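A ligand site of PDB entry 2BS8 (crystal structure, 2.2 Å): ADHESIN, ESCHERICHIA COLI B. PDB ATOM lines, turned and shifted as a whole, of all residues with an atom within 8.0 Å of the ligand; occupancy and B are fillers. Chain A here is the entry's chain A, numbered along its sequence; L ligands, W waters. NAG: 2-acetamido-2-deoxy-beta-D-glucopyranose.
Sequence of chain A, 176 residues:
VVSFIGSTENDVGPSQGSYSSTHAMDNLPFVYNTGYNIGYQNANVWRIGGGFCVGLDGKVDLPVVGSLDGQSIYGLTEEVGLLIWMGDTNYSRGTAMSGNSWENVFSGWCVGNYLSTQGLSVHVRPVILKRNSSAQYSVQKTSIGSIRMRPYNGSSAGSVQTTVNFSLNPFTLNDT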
ATOM      1  N   GLN A  41      15.903  22.931 -20.419  1.00  0.00           N
ATOM      2  CA  GLN A  41      14.673  22.340 -20.901  1.00  0.00           C
ATOM      3  C   GLN A  41      14.304  21.048 -20.180  1.00  0.00           C
ATOM      4  O   GLN A  41      15.053  20.070 -20.216  1.00  0.00           O
ATOM      5  CB  GLN A  41      14.802  22.085 -22.399  1.00  0.00           C
ATOM      6  CG  GLN A  41      13.557  21.626 -23.113  1.00  0.00           C
ATOM      7  CD  GLN A  41      13.792  21.497 -24.607  1.00  0.00           C
ATOM      8  OE1 GLN A  41      14.812  20.929 -25.023  1.00  0.00           O
ATOM      9  NE2 GLN A  41      12.872  22.021 -25.410  1.00  0.00           N
ATOM     10  N   ASN A  42      13.165  21.058 -19.512  1.00  0.00           N
ATOM     11  CA  ASN A  42      12.671  19.881 -18.801  1.00  0.00           C
ATOM     12  C   ASN A  42      11.173  19.818 -19.109  1.00  0.00           C
ATOM     13  O   ASN A  42      10.371  20.524 -18.489  1.00  0.00           O
ATOM     14  CB  ASN A  42      12.880  20.022 -17.292  1.00  0.00           C
ATOM     15  CG  ASN A  42      12.569  18.734 -16.530  1.00  0.00           C
ATOM     16  OD1 ASN A  42      11.640  18.010 -16.887  1.00  0.00           O
ATOM     17  ND2 ASN A  42      13.333  18.459 -15.476  1.00  0.00           N
ATOM     18  N   ALA A  43      10.811  19.000 -20.084  1.00  0.00           N
ATOM     19  CA  ALA A  43       9.417  18.856 -20.470  1.00  0.00           C
ATOM     20  C   ALA A  43       8.618  18.119 -19.386  1.00  0.00           C
ATOM     21  O   ALA A  43       7.434  17.844 -19.572  1.00  0.00           O
ATOM     22  CB  ALA A  43       9.317  18.096 -21.783  1.00  0.00           C
ATOM     23  N   ASN A  44       9.272  17.813 -18.272  1.00  0.00           N
ATOM     24  CA  ASN A  44       8.632  17.095 -17.175  1.00  0.00           C
ATOM     25  C   ASN A  44       8.970  17.709 -15.812  1.00  0.00           C
ATOM     26  O   ASN A  44       9.890  17.257 -15.144  1.00  0.00           O
ATOM     27  CB  ASN A  44       9.057  15.622 -17.175  1.00  0.00           C
ATOM     28  CG  ASN A  44       8.836  14.937 -18.517  1.00  0.00           C
ATOM     29  OD1 ASN A  44       7.734  14.980 -19.085  1.00  0.00           O
ATOM     30  ND2 ASN A  44       9.889  14.303 -19.031  1.00  0.00           N
ATOM     31  N   VAL A  45       8.219  18.735 -15.419  1.00  0.00           N
ATOM     32  CA  VAL A  45       8.424  19.428 -14.145  1.00  0.00           C
ATOM     33  C   VAL A  45       7.204  19.299 -13.215  1.00  0.00           C
ATOM     34  O   VAL A  45       7.336  19.313 -11.988  1.00  0.00           O
ATOM     35  CB  VAL A  45       8.785  20.937 -14.412  1.00  0.00           C
ATOM     36  CG1 VAL A  45       8.732  21.759 -13.122  1.00  0.00           C
ATOM     37  CG2 VAL A  45      10.176  21.027 -15.020  1.00  0.00           C
ATOM     38  N   TRP A  46       6.011  19.168 -13.804  1.00  0.00           N
ATOM     39  CA  TRP A  46       4.774  19.008 -13.028  1.00  0.00           C
ATOM     40  C   TRP A  46       3.892  17.927 -13.640  1.00  0.00           C
ATOM     41  O   TRP A  46       3.623  17.933 -14.848  1.00  0.00           O
ATOM     42  CB  TRP A  46       3.977  20.319 -12.991  1.00  0.00           C
ATOM     43  CG  TRP A  46       4.597  21.415 -12.177  1.00  0.00           C
ATOM     44  CD1 TRP A  46       4.681  21.493 -10.806  1.00  0.00           C
ATOM     45  CD2 TRP A  46       5.288  22.571 -12.689  1.00  0.00           C
ATOM     46  NE1 TRP A  46       5.391  22.618 -10.443  1.00  0.00           N
ATOM     47  CE2 TRP A  46       5.781  23.293 -11.570  1.00  0.00           C
ATOM     48  CE3 TRP A  46       5.550  23.054 -13.973  1.00  0.00           C
ATOM     49  CZ2 TRP A  46       6.511  24.471 -11.713  1.00  0.00           C
ATOM     50  CZ3 TRP A  46       6.280  24.231 -14.117  1.00  0.00           C
ATOM     51  CH2 TRP A  46       6.751  24.929 -12.990  1.00  0.00           C
ATOM     52  N   ILE A  48       0.280  16.380 -14.145  1.00  0.00           N
ATOM     53  CA  ILE A  48      -1.088  16.851 -13.998  1.00  0.00           C
ATOM     54  C   ILE A  48      -2.098  15.858 -14.529  1.00  0.00           C
ATOM     55  O   ILE A  48      -1.791  15.023 -15.381  1.00  0.00           O
ATOM     56  CB  ILE A  48      -1.278  18.193 -14.734  1.00  0.00           C
ATOM     57  CG1 ILE A  48      -1.280  17.952 -16.251  1.00  0.00           C
ATOM     58  CG2 ILE A  48      -0.174  19.166 -14.311  1.00  0.00           C
ATOM     59  CD1 ILE A  48      -1.297  19.202 -17.095  1.00  0.00           C
ATOM     60  N   VAL A  54      -2.992  24.471 -16.431  1.00  0.00           N
ATOM     61  CA  VAL A  54      -1.824  25.203 -15.957  1.00  0.00           C
ATOM     62  C   VAL A  54      -1.163  26.106 -17.001  1.00  0.00           C
ATOM     63  O   VAL A  54      -1.146  25.796 -18.195  1.00  0.00           O
ATOM     64  CB  VAL A  54      -0.741  24.251 -15.386  1.00  0.00           C
ATOM     65  CG1 VAL A  54      -0.355  23.195 -16.414  1.00  0.00           C
ATOM     66  CG2 VAL A  54       0.498  25.051 -15.018  1.00  0.00           C
ATOM     67  N   LEU A  56       2.220  29.345 -17.429  1.00  0.00           N
ATOM     68  CA  LEU A  56       3.565  29.550 -16.928  1.00  0.00           C
ATOM     69  C   LEU A  56       4.021  30.998 -16.769  1.00  0.00           C
ATOM     70  O   LEU A  56       3.898  31.813 -17.684  1.00  0.00           O
ATOM     71  CB  LEU A  56       4.575  28.797 -17.804  1.00  0.00           C
ATOM     72  CG  LEU A  56       4.519  27.267 -17.752  1.00  0.00           C
ATOM     73  CD1 LEU A  56       5.710  26.699 -18.505  1.00  0.00           C
ATOM     74  CD2 LEU A  56       4.535  26.787 -16.308  1.00  0.00           C
ATOM     75  N   GLY A  87       9.363  30.254 -20.946  1.00  0.00           N
ATOM     76  CA  GLY A  87       8.065  29.800 -21.408  1.00  0.00           C
ATOM     77  C   GLY A  87       7.903  28.298 -21.280  1.00  0.00           C
ATOM     78  O   GLY A  87       8.565  27.652 -20.454  1.00  0.00           O
ATOM     79  N   ASP A  88       7.035  27.736 -22.119  1.00  0.00           N
ATOM     80  CA  ASP A  88       6.761  26.298 -22.130  1.00  0.00           C
ATOM     81  C   ASP A  88       7.893  25.451 -22.716  1.00  0.00           C
ATOM     82  O   ASP A  88       8.934  25.952 -23.119  1.00  0.00           O
ATOM     83  CB  ASP A  88       5.461  26.027 -22.886  1.00  0.00           C
ATOM     84  CG  ASP A  88       5.010  24.573 -22.790  1.00  0.00           C
ATOM     85  OD1 ASP A  88       4.868  24.040 -21.678  1.00  0.00           O
ATOM     86  OD2 ASP A  88       4.781  23.967 -23.845  1.00  0.00           O
ATOM     87  N   THR A  89       7.642  24.141 -22.761  1.00  0.00           N
ATOM     88  CA  THR A  89       8.602  23.155 -23.257  1.00  0.00           C
ATOM     89  C   THR A  89       9.380  23.496 -24.548  1.00  0.00           C
ATOM     90  O   THR A  89      10.520  23.934 -24.487  1.00  0.00           O
ATOM     91  CB  THR A  89       7.886  21.801 -23.414  1.00  0.00           C
ATOM     92  OG1 THR A  89       7.205  21.508 -22.190  1.00  0.00           O
ATOM     93  CG2 THR A  89       8.893  20.673 -23.731  1.00  0.00           C
ATOM     94  N   ASN A  90       8.783  23.285 -25.718  1.00  0.00           N
ATOM     95  CA  ASN A  90       9.483  23.586 -26.972  1.00  0.00           C
ATOM     96  C   ASN A  90      10.228  24.924 -26.886  1.00  0.00           C
ATOM     97  O   ASN A  90       9.602  25.969 -26.763  1.00  0.00           O
ATOM     98  N   ARG A  93       8.978  27.980 -28.383  1.00  0.00           N
ATOM     99  CA  ARG A  93       7.789  28.569 -27.780  1.00  0.00           C
ATOM    100  C   ARG A  93       8.112  29.671 -26.765  1.00  0.00           C
ATOM    101  O   ARG A  93       7.217  30.198 -26.103  1.00  0.00           O
ATOM    102  CB  ARG A  93       6.968  27.473 -27.097  1.00  0.00           C
ATOM    103  CG  ARG A  93       6.608  26.297 -27.999  1.00  0.00           C
ATOM    104  CD  ARG A  93       5.256  26.500 -28.668  1.00  0.00           C
ATOM    105  NE  ARG A  93       4.971  25.528 -29.722  1.00  0.00           N
ATOM    106  CZ  ARG A  93       4.754  24.233 -29.525  1.00  0.00           C
ATOM    107  NH1 ARG A  93       4.503  23.446 -30.560  1.00  0.00           N
ATOM    108  NH2 ARG A  93       4.782  23.716 -28.295  1.00  0.00           N
ATOM    109  N   PHE A 106       3.653  31.599 -20.874  1.00  0.00           N
ATOM    110  CA  PHE A 106       2.937  30.543 -21.593  1.00  0.00           C
ATOM    111  C   PHE A 106       1.466  30.618 -21.226  1.00  0.00           C
ATOM    112  O   PHE A 106       1.125  30.563 -20.058  1.00  0.00           O
ATOM    113  CB  PHE A 106       3.508  29.154 -21.244  1.00  0.00           C
ATOM    114  CG  PHE A 106       2.628  27.999 -21.639  1.00  0.00           C
ATOM    115  CD1 PHE A 106       1.999  27.978 -22.876  1.00  0.00           C
ATOM    116  CD2 PHE A 106       2.452  26.928 -20.773  1.00  0.00           C
ATOM    117  CE1 PHE A 106       1.221  26.892 -23.254  1.00  0.00           C
ATOM    118  CE2 PHE A 106       1.681  25.831 -21.137  1.00  0.00           C
ATOM    119  CZ  PHE A 106       1.055  25.812 -22.387  1.00  0.00           C
ATOM    120  N   GLY A 108      -0.689  28.557 -21.282  1.00  0.00           N
ATOM    121  CA  GLY A 108      -1.125  27.369 -20.568  1.00  0.00           C
ATOM    122  C   GLY A 108      -2.095  26.523 -21.360  1.00  0.00           C
ATOM    123  O   GLY A 108      -2.433  26.845 -22.501  1.00  0.00           O
ATOM    124  N   TRP A 109      -2.554  25.439 -20.731  1.00  0.00           N
ATOM    125  CA  TRP A 109      -3.506  24.521 -21.355  1.00  0.00           C
ATOM    126  C   TRP A 109      -4.254  23.759 -20.250  1.00  0.00           C
ATOM    127  O   TRP A 109      -3.965  23.909 -19.066  1.00  0.00           O
ATOM    128  CB  TRP A 109      -2.793  23.537 -22.274  1.00  0.00           C
ATOM    129  CG  TRP A 109      -1.892  22.580 -21.531  1.00  0.00           C
ATOM    130  CD1 TRP A 109      -0.846  22.905 -20.711  1.00  0.00           C
ATOM    131  CD2 TRP A 109      -1.925  21.149 -21.592  1.00  0.00           C
ATOM    132  NE1 TRP A 109      -0.228  21.773 -20.264  1.00  0.00           N
ATOM    133  CE2 TRP A 109      -0.860  20.688 -20.787  1.00  0.00           C
ATOM    134  CE3 TRP A 109      -2.734  20.227 -22.253  1.00  0.00           C
ATOM    135  CZ2 TRP A 109      -0.602  19.321 -20.617  1.00  0.00           C
ATOM    136  CZ3 TRP A 109      -2.473  18.872 -22.088  1.00  0.00           C
ATOM    137  CH2 TRP A 109      -1.419  18.432 -21.274  1.00  0.00           C
ATOM    138  N   CYS A 110      -5.218  22.950 -20.671  1.00  0.00           N
ATOM    139  CA  CYS A 110      -6.023  22.162 -19.749  1.00  0.00           C
ATOM    140  C   CYS A 110      -5.994  20.689 -20.139  1.00  0.00           C
ATOM    141  O   CYS A 110      -6.742  20.284 -21.025  1.00  0.00           O
ATOM    142  CB  CYS A 110      -7.479  22.607 -19.785  1.00  0.00           C
ATOM    143  SG  CYS A 110      -7.937  24.254 -19.132  1.00  0.00           S
ATOM    144  N   VAL A 111      -5.148  19.894 -19.486  1.00  0.00           N
ATOM    145  CA  VAL A 111      -5.057  18.465 -19.762  1.00  0.00           C
ATOM    146  C   VAL A 111      -6.425  17.782 -19.680  1.00  0.00           C
ATOM    147  O   VAL A 111      -7.395  18.348 -19.181  1.00  0.00           O
ATOM    148  CB  VAL A 111      -4.118  17.770 -18.746  1.00  0.00           C
ATOM    149  CG1 VAL A 111      -4.706  17.896 -17.333  1.00  0.00           C
ATOM    150  CG2 VAL A 111      -3.921  16.302 -19.107  1.00  0.00           C
ATOM    151  N   LEU A 115      -3.400  11.237 -17.302  1.00  0.00           N
ATOM    152  CA  LEU A 115      -2.138  11.745 -16.738  1.00  0.00           C
ATOM    153  C   LEU A 115      -1.113  12.210 -17.740  1.00  0.00           C
ATOM    154  O   LEU A 115      -0.620  11.425 -18.539  1.00  0.00           O
ATOM    155  CB  LEU A 115      -1.486  10.697 -15.841  1.00  0.00           C
ATOM    156  CG  LEU A 115      -2.134  10.504 -14.473  1.00  0.00           C
ATOM    157  CD1 LEU A 115      -2.549  11.874 -13.938  1.00  0.00           C
ATOM    158  CD2 LEU A 115      -3.342   9.591 -14.588  1.00  0.00           C
ATOM    159  N   SER A 116      -0.781  13.496 -17.674  1.00  0.00           N
ATOM    160  CA  SER A 116       0.206  14.096 -18.563  1.00  0.00           C
ATOM    161  C   SER A 116       1.291  14.771 -17.691  1.00  0.00           C
ATOM    162  O   SER A 116       1.423  14.457 -16.519  1.00  0.00           O
ATOM    163  CB  SER A 116      -0.472  15.137 -19.451  1.00  0.00           C
ATOM    164  OG  SER A 116       0.448  15.747 -20.353  1.00  0.00           O
ATOM    165  N   THR A 117       2.062  15.684 -18.273  1.00  0.00           N
ATOM    166  CA  THR A 117       3.105  16.386 -17.537  1.00  0.00           C
ATOM    167  C   THR A 117       3.211  17.803 -18.090  1.00  0.00           C
ATOM    168  O   THR A 117       2.778  18.067 -19.215  1.00  0.00           O
ATOM    169  CB  THR A 117       4.483  15.657 -17.646  1.00  0.00           C
ATOM    170  OG1 THR A 117       5.027  15.804 -18.970  1.00  0.00           O
ATOM    171  CG2 THR A 117       4.319  14.164 -17.371  1.00  0.00           C
ATOM    172  N   GLN A 118       3.714  18.730 -17.282  1.00  0.00           N
ATOM    173  CA  GLN A 118       3.858  20.115 -17.715  1.00  0.00           C
ATOM    174  C   GLN A 118       5.322  20.488 -17.625  1.00  0.00           C
ATOM    175  O   GLN A 118       6.009  20.155 -16.646  1.00  0.00           O
ATOM    176  CB  GLN A 118       3.003  21.077 -16.850  1.00  0.00           C
ATOM    177  CG  GLN A 118       3.407  22.551 -16.961  1.00  0.00           C
ATOM    178  CD  GLN A 118       3.117  23.180 -18.324  1.00  0.00           C
ATOM    179  OE1 GLN A 118       1.995  23.081 -18.828  1.00  0.00           O
ATOM    180  NE2 GLN A 118       4.110  23.843 -18.917  1.00  0.00           N
ATOM    181  N   GLY A 119       5.797  21.191 -18.649  1.00  0.00           N
ATOM    182  CA  GLY A 119       7.186  21.574 -18.719  1.00  0.00           C
ATOM    183  C   GLY A 119       7.489  23.043 -18.837  1.00  0.00           C
ATOM    184  O   GLY A 119       6.612  23.905 -18.772  1.00  0.00           O
ATOM    185  N   LEU A 120       8.774  23.322 -19.060  1.00  0.00           N
ATOM    186  CA  LEU A 120       9.268  24.685 -19.168  1.00  0.00           C
ATOM    187  C   LEU A 120      10.619  24.703 -19.868  1.00  0.00           C
ATOM    188  O   LEU A 120      11.277  23.672 -19.996  1.00  0.00           O
ATOM    189  CB  LEU A 120       9.405  25.254 -17.751  1.00  0.00           C
ATOM    190  CG  LEU A 120      10.203  24.359 -16.794  1.00  0.00           C
ATOM    191  CD1 LEU A 120      11.662  24.804 -16.782  1.00  0.00           C
ATOM    192  CD2 LEU A 120       9.613  24.417 -15.421  1.00  0.00           C
ATOM    193  N   SER A 121      11.033  25.890 -20.310  1.00  0.00           N
ATOM    194  CA  SER A 121      12.290  26.005 -21.008  1.00  0.00           C
ATOM    195  C   SER A 121      12.802  27.431 -20.978  1.00  0.00           C
ATOM    196  O   SER A 121      12.027  28.388 -21.097  1.00  0.00           O
ATOM    197  CB  SER A 121      12.123  25.567 -22.485  1.00  0.00           C
ATOM    198  OG  SER A 121      11.308  26.472 -23.218  1.00  0.00           O
HETATM  199  C1  NAG L   1       2.683  18.080 -22.247  1.00  0.00           C
HETATM  200  C2  NAG L   1       4.215  18.011 -22.337  1.00  0.00           C
HETATM  201  C3  NAG L   1       4.807  19.101 -21.472  1.00  0.00           C
HETATM  202  C4  NAG L   1       4.262  20.483 -21.868  1.00  0.00           C
HETATM  203  C5  NAG L   1       2.717  20.458 -21.873  1.00  0.00           C
HETATM  204  C6  NAG L   1       2.084  21.721 -22.429  1.00  0.00           C
HETATM  205  C7  NAG L   1       4.973  15.757 -22.761  1.00  0.00           C
HETATM  206  C8  NAG L   1       5.834  16.090 -23.962  1.00  0.00           C
HETATM  207  N2  NAG L   1       4.735  16.731 -21.889  1.00  0.00           N
HETATM  208  O1  NAG L   1       2.110  17.128 -23.081  1.00  0.00           O
HETATM  209  O3  NAG L   1       6.216  19.094 -21.587  1.00  0.00           O
HETATM  210  O4  NAG L   1       4.718  21.432 -20.920  1.00  0.00           O
HETATM  211  O5  NAG L   1       2.220  19.371 -22.675  1.00  0.00           O
HETATM  212  O6  NAG L   1       2.471  21.946 -23.774  1.00  0.00           O
HETATM  213  O7  NAG L   1       4.542  14.612 -22.608  1.00  0.00           O
HETATM  214  O   HOH W   1      -0.463  19.782 -24.833  1.00  0.00           O
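O1 of the ligand is in hydrogen-bond range of OG of Ser 116 (3.5 Å).
The side-chain amide nitrogen (NE2) of Gln 118 sits at hydrogen-bond distance from an oxygen (O4) of the ligand, 3.2 Å away.
The backbone NH (N) of Gly 119 lies within hydrogen-bond range of an oxygen (O4) of the ligand.
The backbone carbonyl oxygen (O) of Ala 43 is in hydrogen-bond range of an oxygen (O3) of the ligand (2.7 Å).
OG1 of Thr 89 lies within hydrogen-bond range of O3 of the ligand.
OD1 of Asp 88 lies within hydrogen-bond range of O4 of the ligand (2.7 Å).
A nitrogen (N2) of the ligand lies within hydrogen-bond range of the side-chain hydroxyl (OG1) of Thr 117 (3.1 Å).
Residues that only touch the ligand: Trp 109.
Of the 26 residues printed, 8 come within 4 Å of the ligand.
Along chain A the residues within 4 Å of the ligand span positions 43 to 119.
The nearest printed residue that does not touch the ligand is Phe 106 (4.2 Å).
O of Thr 89 sits at hydrogen-bond distance from NE2 of Gln 41, at 3.2 Å.
O of Thr 89 sits at hydrogen-bond distance from OG of Ser 121 (2.9 Å).
OD1 of Asp 88 sits at hydrogen-bond distance from NE2 of Gln 118 (2.9 Å).
The backbone carbonyl oxygen (O) of Gln 118 sits at hydrogen-bond distance from the backbone NH (N) of Val 45.
The side-chain hydroxyl of Thr 117 is in hydrogen-bond range of the side-chain amide oxygen of Asn 44, 2.8 Å away.
The backbone carbonyl oxygen (O) of Ala 43 is in hydrogen-bond range of the side-chain hydroxyl (OG1) of Thr 117.
O of Trp 46 is in hydrogen-bond range of N of Gln 118, 2.6 Å away.
OG of Ser 121 sits at hydrogen-bond distance from O of Asp 88, 2.4 Å away.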
